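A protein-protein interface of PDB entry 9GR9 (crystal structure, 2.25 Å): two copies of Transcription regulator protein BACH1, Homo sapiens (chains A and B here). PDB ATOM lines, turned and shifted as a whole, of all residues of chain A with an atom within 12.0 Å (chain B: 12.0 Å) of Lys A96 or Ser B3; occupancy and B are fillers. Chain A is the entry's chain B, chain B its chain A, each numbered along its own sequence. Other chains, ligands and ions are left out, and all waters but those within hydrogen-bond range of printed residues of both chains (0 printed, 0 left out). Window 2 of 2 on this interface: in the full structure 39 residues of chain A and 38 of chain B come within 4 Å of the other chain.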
ATOM      1  N   LYS A  78     -17.922   7.604   4.774  1.00  0.00           N
ATOM      2  CA  LYS A  78     -17.627   8.149   6.095  1.00  0.00           C
ATOM      3  C   LYS A  78     -18.357   9.463   6.337  1.00  0.00           C
ATOM      4  O   LYS A  78     -18.649   9.807   7.488  1.00  0.00           O
ATOM      5  CB  LYS A  78     -16.116   8.332   6.253  1.00  0.00           C
ATOM      6  CG  LYS A  78     -15.672   8.714   7.652  1.00  0.00           C
ATOM      7  CD  LYS A  78     -14.169   8.542   7.819  1.00  0.00           C
ATOM      8  CE  LYS A  78     -13.393   9.455   6.887  1.00  0.00           C
ATOM      9  NZ  LYS A  78     -11.922   9.296   7.064  1.00  0.00           N
ATOM     10  N   GLY A  79     -18.673  10.199   5.276  1.00  0.00           N
ATOM     11  CA  GLY A  79     -19.381  11.454   5.418  1.00  0.00           C
ATOM     12  C   GLY A  79     -20.874  11.339   5.184  1.00  0.00           C
ATOM     13  O   GLY A  79     -21.667  12.023   5.840  1.00  0.00           O
ATOM     14  N   PRO A  82     -23.341   9.292   8.326  1.00  0.00           N
ATOM     15  CA  PRO A  82     -23.893  10.069   9.447  1.00  0.00           C
ATOM     16  C   PRO A  82     -25.030  10.989   9.040  1.00  0.00           C
ATOM     17  O   PRO A  82     -25.877  11.319   9.880  1.00  0.00           O
ATOM     18  CB  PRO A  82     -22.680  10.861   9.955  1.00  0.00           C
ATOM     19  CG  PRO A  82     -21.511  10.046   9.555  1.00  0.00           C
ATOM     20  CD  PRO A  82     -21.878   9.450   8.230  1.00  0.00           C
ATOM     21  N   LEU A  92     -27.434  13.506  14.903  1.00  0.00           N
ATOM     22  CA  LEU A  92     -26.217  13.718  14.131  1.00  0.00           C
ATOM     23  C   LEU A  92     -25.019  13.530  15.050  1.00  0.00           C
ATOM     24  O   LEU A  92     -24.844  14.293  16.005  1.00  0.00           O
ATOM     25  CB  LEU A  92     -26.204  15.113  13.501  1.00  0.00           C
ATOM     26  CG  LEU A  92     -24.978  15.495  12.669  1.00  0.00           C
ATOM     27  CD1 LEU A  92     -24.828  14.571  11.472  1.00  0.00           C
ATOM     28  CD2 LEU A  92     -25.072  16.943  12.221  1.00  0.00           C
ATOM     29  N   ILE A  93     -24.200  12.524  14.760  1.00  0.00           N
ATOM     30  CA  ILE A  93     -23.061  12.162  15.597  1.00  0.00           C
ATOM     31  C   ILE A  93     -21.787  12.553  14.862  1.00  0.00           C
ATOM     32  O   ILE A  93     -21.494  12.021  13.784  1.00  0.00           O
ATOM     33  CB  ILE A  93     -23.065  10.665  15.938  1.00  0.00           C
ATOM     34  CG1 ILE A  93     -24.425  10.247  16.497  1.00  0.00           C
ATOM     35  CG2 ILE A  93     -21.960  10.345  16.931  1.00  0.00           C
ATOM     36  CD1 ILE A  93     -24.520   8.773  16.832  1.00  0.00           C
ATOM     37  N   LEU A  94     -21.030  13.478  15.443  1.00  0.00           N
ATOM     38  CA  LEU A  94     -19.791  13.969  14.859  1.00  0.00           C
ATOM     39  C   LEU A  94     -18.601  13.582  15.728  1.00  0.00           C
ATOM     40  O   LEU A  94     -18.728  13.401  16.943  1.00  0.00           O
ATOM     41  CB  LEU A  94     -19.829  15.493  14.688  1.00  0.00           C
ATOM     42  CG  LEU A  94     -20.915  16.071  13.779  1.00  0.00           C
ATOM     43  CD1 LEU A  94     -20.848  17.590  13.763  1.00  0.00           C
ATOM     44  CD2 LEU A  94     -20.791  15.510  12.373  1.00  0.00           C
ATOM     45  N   SER A  95     -17.438  13.458  15.090  1.00  0.00           N
ATOM     46  CA  SER A  95     -16.197  13.169  15.794  1.00  0.00           C
ATOM     47  C   SER A  95     -15.046  13.781  15.012  1.00  0.00           C
ATOM     48  O   SER A  95     -15.188  14.136  13.841  1.00  0.00           O
ATOM     49  CB  SER A  95     -15.984  11.661  15.977  1.00  0.00           C
ATOM     50  OG  SER A  95     -15.743  11.023  14.734  1.00  0.00           O
ATOM     51  N   LYS A  96     -13.892  13.890  15.674  1.00  0.00           N
ATOM     52  CA  LYS A  96     -12.717  14.480  15.040  1.00  0.00           C
ATOM     53  C   LYS A  96     -12.232  13.678  13.838  1.00  0.00           C
ATOM     54  O   LYS A  96     -11.427  14.194  13.054  1.00  0.00           O
ATOM     55  CB  LYS A  96     -11.587  14.621  16.063  1.00  0.00           C
ATOM     56  N   GLU A  97     -12.706  12.441  13.677  1.00  0.00           N
ATOM     57  CA  GLU A  97     -12.354  11.581  12.554  1.00  0.00           C
ATOM     58  C   GLU A  97     -13.225  11.833  11.329  1.00  0.00           C
ATOM     59  O   GLU A  97     -12.728  11.782  10.199  1.00  0.00           O
ATOM     60  CB  GLU A  97     -12.473  10.109  12.965  1.00  0.00           C
ATOM     61  CG  GLU A  97     -11.595   9.710  14.140  1.00  0.00           C
ATOM     62  CD  GLU A  97     -11.785   8.259  14.555  1.00  0.00           C
ATOM     63  OE1 GLU A  97     -12.712   7.602  14.037  1.00  0.00           O
ATOM     64  OE2 GLU A  97     -11.005   7.774  15.402  1.00  0.00           O
ATOM     65  N   ASN A  98     -14.517  12.099  11.525  1.00  0.00           N
ATOM     66  CA  ASN A  98     -15.457  12.230  10.420  1.00  0.00           C
ATOM     67  C   ASN A  98     -16.006  13.640  10.247  1.00  0.00           C
ATOM     68  O   ASN A  98     -16.796  13.868   9.326  1.00  0.00           O
ATOM     69  CB  ASN A  98     -16.623  11.248  10.601  1.00  0.00           C
ATOM     70  CG  ASN A  98     -17.573  11.663  11.713  1.00  0.00           C
ATOM     71  OD1 ASN A  98     -17.186  12.350  12.658  1.00  0.00           O
ATOM     72  ND2 ASN A  98     -18.827  11.242  11.603  1.00  0.00           N
ATOM     73  N   VAL A  99     -15.614  14.590  11.100  1.00  0.00           N
ATOM     74  CA  VAL A  99     -16.192  15.931  11.034  1.00  0.00           C
ATOM     75  C   VAL A  99     -15.875  16.592   9.697  1.00  0.00           C
ATOM     76  O   VAL A  99     -16.697  17.335   9.144  1.00  0.00           O
ATOM     77  CB  VAL A  99     -15.705  16.783  12.223  1.00  0.00           C
ATOM     78  CG1 VAL A  99     -14.188  16.838  12.262  1.00  0.00           C
ATOM     79  CG2 VAL A  99     -16.297  18.183  12.164  1.00  0.00           C
ATOM     80  N   ASP A 100     -14.692  16.318   9.145  1.00  0.00           N
ATOM     81  CA  ASP A 100     -14.302  16.935   7.882  1.00  0.00           C
ATOM     82  C   ASP A 100     -15.102  16.361   6.720  1.00  0.00           C
ATOM     83  O   ASP A 100     -15.615  17.107   5.877  1.00  0.00           O
ATOM     84  CB  ASP A 100     -12.803  16.749   7.653  1.00  0.00           C
ATOM     85  CG  ASP A 100     -11.968  17.302   8.789  1.00  0.00           C
ATOM     86  OD1 ASP A 100     -12.245  18.437   9.235  1.00  0.00           O
ATOM     87  OD2 ASP A 100     -11.043  16.597   9.245  1.00  0.00           O
ATOM     88  N   GLU A 101     -15.220  15.033   6.659  1.00  0.00           N
ATOM     89  CA  GLU A 101     -15.943  14.403   5.560  1.00  0.00           C
ATOM     90  C   GLU A 101     -17.447  14.629   5.668  1.00  0.00           C
ATOM     91  O   GLU A 101     -18.138  14.688   4.643  1.00  0.00           O
ATOM     92  CB  GLU A 101     -15.628  12.909   5.518  1.00  0.00           C
ATOM     93  CG  GLU A 101     -14.170  12.596   5.223  1.00  0.00           C
ATOM     94  CD  GLU A 101     -13.798  12.860   3.777  1.00  0.00           C
ATOM     95  OE1 GLU A 101     -14.693  12.785   2.908  1.00  0.00           O
ATOM     96  OE2 GLU A 101     -12.611  13.143   3.507  1.00  0.00           O
ATOM     97  N   VAL A 102     -17.973  14.757   6.889  1.00  0.00           N
ATOM     98  CA  VAL A 102     -19.396  15.037   7.053  1.00  0.00           C
ATOM     99  C   VAL A 102     -19.704  16.480   6.673  1.00  0.00           C
ATOM    100  O   VAL A 102     -20.710  16.759   6.009  1.00  0.00           O
ATOM    101  CB  VAL A 102     -19.846  14.715   8.491  1.00  0.00           C
ATOM    102  CG1 VAL A 102     -21.230  15.279   8.756  1.00  0.00           C
ATOM    103  CG2 VAL A 102     -19.844  13.213   8.719  1.00  0.00           C
ATOM    104  N   CYS A 103     -18.842  17.418   7.076  1.00  0.00           N
ATOM    105  CA  CYS A 103     -19.036  18.815   6.697  1.00  0.00           C
ATOM    106  C   CYS A 103     -19.034  18.982   5.183  1.00  0.00           C
ATOM    107  O   CYS A 103     -19.735  19.848   4.645  1.00  0.00           O
ATOM    108  CB  CYS A 103     -17.954  19.687   7.335  1.00  0.00           C
ATOM    109  SG  CYS A 103     -18.092  21.448   6.952  1.00  0.00           S
ATOM    110  N   LYS A 104     -18.259  18.155   4.478  1.00  0.00           N
ATOM    111  CA  LYS A 104     -18.231  18.223   3.021  1.00  0.00           C
ATOM    112  C   LYS A 104     -19.566  17.790   2.424  1.00  0.00           C
ATOM    113  O   LYS A 104     -20.100  18.449   1.524  1.00  0.00           O
ATOM    114  CB  LYS A 104     -17.092  17.360   2.481  1.00  0.00           C
ATOM    115  N   CYS A 118     -21.950  23.688  14.747  1.00  0.00           N
ATOM    116  CA  CYS A 118     -21.505  22.498  15.464  1.00  0.00           C
ATOM    117  C   CYS A 118     -20.219  21.903  14.894  1.00  0.00           C
ATOM    118  O   CYS A 118     -19.846  20.788  15.274  1.00  0.00           O
ATOM    119  CB  CYS A 118     -22.610  21.440  15.469  1.00  0.00           C
ATOM    120  SG  CYS A 118     -23.134  20.879  13.828  1.00  0.00           S
ATOM    121  N   PHE A 119     -19.543  22.610  13.995  1.00  0.00           N
ATOM    122  CA  PHE A 119     -18.279  22.141  13.439  1.00  0.00           C
ATOM    123  C   PHE A 119     -17.103  22.898  14.050  1.00  0.00           C
ATOM    124  O   PHE A 119     -16.469  22.420  14.991  1.00  0.00           O
ATOM    125  CB  PHE A 119     -18.272  22.294  11.915  1.00  0.00           C
ATOM    126  CG  PHE A 119     -19.310  21.459  11.216  1.00  0.00           C
ATOM    127  CD1 PHE A 119     -19.038  20.150  10.855  1.00  0.00           C
ATOM    128  CD2 PHE A 119     -20.556  21.986  10.915  1.00  0.00           C
ATOM    129  CE1 PHE A 119     -19.990  19.381  10.211  1.00  0.00           C
ATOM    130  CE2 PHE A 119     -21.511  21.222  10.271  1.00  0.00           C
ATOM    131  CZ  PHE A 119     -21.228  19.917   9.918  1.00  0.00           C
ATOM    132  N   SER B   3     -13.383  11.826  21.399  1.00  0.00           N
ATOM    133  CA  SER B   3     -14.160  13.056  21.491  1.00  0.00           C
ATOM    134  C   SER B   3     -15.298  13.039  20.473  1.00  0.00           C
ATOM    135  O   SER B   3     -15.057  12.994  19.267  1.00  0.00           O
ATOM    136  CB  SER B   3     -13.264  14.275  21.273  1.00  0.00           C
ATOM    137  OG  SER B   3     -13.941  15.474  21.597  1.00  0.00           O
ATOM    138  N   VAL B   4     -16.536  13.074  20.963  1.00  0.00           N
ATOM    139  CA  VAL B   4     -17.725  12.935  20.130  1.00  0.00           C
ATOM    140  C   VAL B   4     -18.712  14.042  20.476  1.00  0.00           C
ATOM    141  O   VAL B   4     -18.899  14.375  21.653  1.00  0.00           O
ATOM    142  CB  VAL B   4     -18.376  11.545  20.310  1.00  0.00           C
ATOM    143  CG1 VAL B   4     -19.710  11.476  19.586  1.00  0.00           C
ATOM    144  CG2 VAL B   4     -17.446  10.451  19.809  1.00  0.00           C
ATOM    145  N   PHE B   5     -19.344  14.610  19.448  1.00  0.00           N
ATOM    146  CA  PHE B   5     -20.386  15.619  19.603  1.00  0.00           C
ATOM    147  C   PHE B   5     -21.662  15.093  18.961  1.00  0.00           C
ATOM    148  O   PHE B   5     -21.680  14.804  17.760  1.00  0.00           O
ATOM    149  CB  PHE B   5     -19.973  16.947  18.964  1.00  0.00           C
ATOM    150  CG  PHE B   5     -18.490  17.192  18.979  1.00  0.00           C
ATOM    151  CD1 PHE B   5     -17.882  17.796  20.067  1.00  0.00           C
ATOM    152  CD2 PHE B   5     -17.703  16.820  17.900  1.00  0.00           C
ATOM    153  CE1 PHE B   5     -16.515  18.022  20.079  1.00  0.00           C
ATOM    154  CE2 PHE B   5     -16.339  17.043  17.909  1.00  0.00           C
ATOM    155  CZ  PHE B   5     -15.746  17.645  18.997  1.00  0.00           C
ATOM    156  N   ALA B   6     -22.722  14.971  19.755  1.00  0.00           N
ATOM    157  CA  ALA B   6     -23.981  14.395  19.303  1.00  0.00           C
ATOM    158  C   ALA B   6     -25.077  15.449  19.360  1.00  0.00           C
ATOM    159  O   ALA B   6     -25.220  16.150  20.368  1.00  0.00           O
ATOM    160  CB  ALA B   6     -24.366  13.182  20.154  1.00  0.00           C
ATOM    161  N   TYR B   7     -25.849  15.552  18.282  1.00  0.00           N
ATOM    162  CA  TYR B   7     -26.949  16.501  18.170  1.00  0.00           C
ATOM    163  C   TYR B   7     -28.255  15.732  18.027  1.00  0.00           C
ATOM    164  O   TYR B   7     -28.346  14.804  17.218  1.00  0.00           O
ATOM    165  CB  TYR B   7     -26.741  17.432  16.969  1.00  0.00           C
ATOM    166  CG  TYR B   7     -27.857  18.425  16.722  1.00  0.00           C
ATOM    167  CD1 TYR B   7     -28.592  18.960  17.772  1.00  0.00           C
ATOM    168  CD2 TYR B   7     -28.174  18.829  15.433  1.00  0.00           C
ATOM    169  CE1 TYR B   7     -29.608  19.867  17.544  1.00  0.00           C
ATOM    170  CE2 TYR B   7     -29.190  19.736  15.194  1.00  0.00           C
ATOM    171  CZ  TYR B   7     -29.905  20.251  16.254  1.00  0.00           C
ATOM    172  OH  TYR B   7     -30.917  21.154  16.024  1.00  0.00           O
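No position is printed for both chains. Of the 9 pairs that touch across the chains among the printed residues, none has its exchanged pair printed and touching as well.
Among the printed residues, pairs that only touch across the chains: Leu A94 with Val B4 (3.4 Å), Leu A92 with Ala B6 (3.4 Å), Leu A92 with Phe B5 (3.7 Å), Ile A93 with Val B4 (3.7 Å), Ser A95 with Ser B3 (3.7 Å), Ile A93 with Phe B5 (3.7 Å) and Lys A96 with Ser B3 (3.9 Å).
O of Phe B5 is in hydrogen-bond range of N of Leu A94 (2.7 Å). The backbone NH (N) of Tyr B7 sits at hydrogen-bond distance from the backbone carbonyl oxygen (O) of Leu A92, 2.8 Å away.
N of Ser A95 lies within hydrogen-bond range of OD1 of Asn A98 (2.7 Å).
Of the printed residues of chain B, Lys A96 touches Ser B3. Ser B3 touches just these residues of chain A: Ser A95 and Lys A96. Of chain B, only Ser B3 comes within 4 Å of Ser A95. No residue of chain B comes within 4 Å of Glu A97. No residue of chain B comes within 4 Å of Asn A98. No residue of chain B comes within 4 Å of Val A99. Printed residues of chain A within 4 Å of Ala B6: Leu A92. Printed residues of chain B within 4 Å of Ile A93: Val B4 (3.7 Å) and Phe B5 (3.7 Å). Val A102 touches none of the printed residues of chain B. The nearest printed residue of chain B that does not touch Leu A94 is Ser B3 (4.4 Å).
Hydrophobic or aromatic side chains of chain A that line the printed part of chain B: Ile A93 and Leu A94. Printed residues of chain B that touch a printed residue of chain A: Ser B3, Val B4, Phe B5, Ala B6 and Tyr B7. Among the printed residues, no Asp or Glu carboxylate lies within 4 Å of a Lys or Arg side-chain nitrogen of the other chain.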
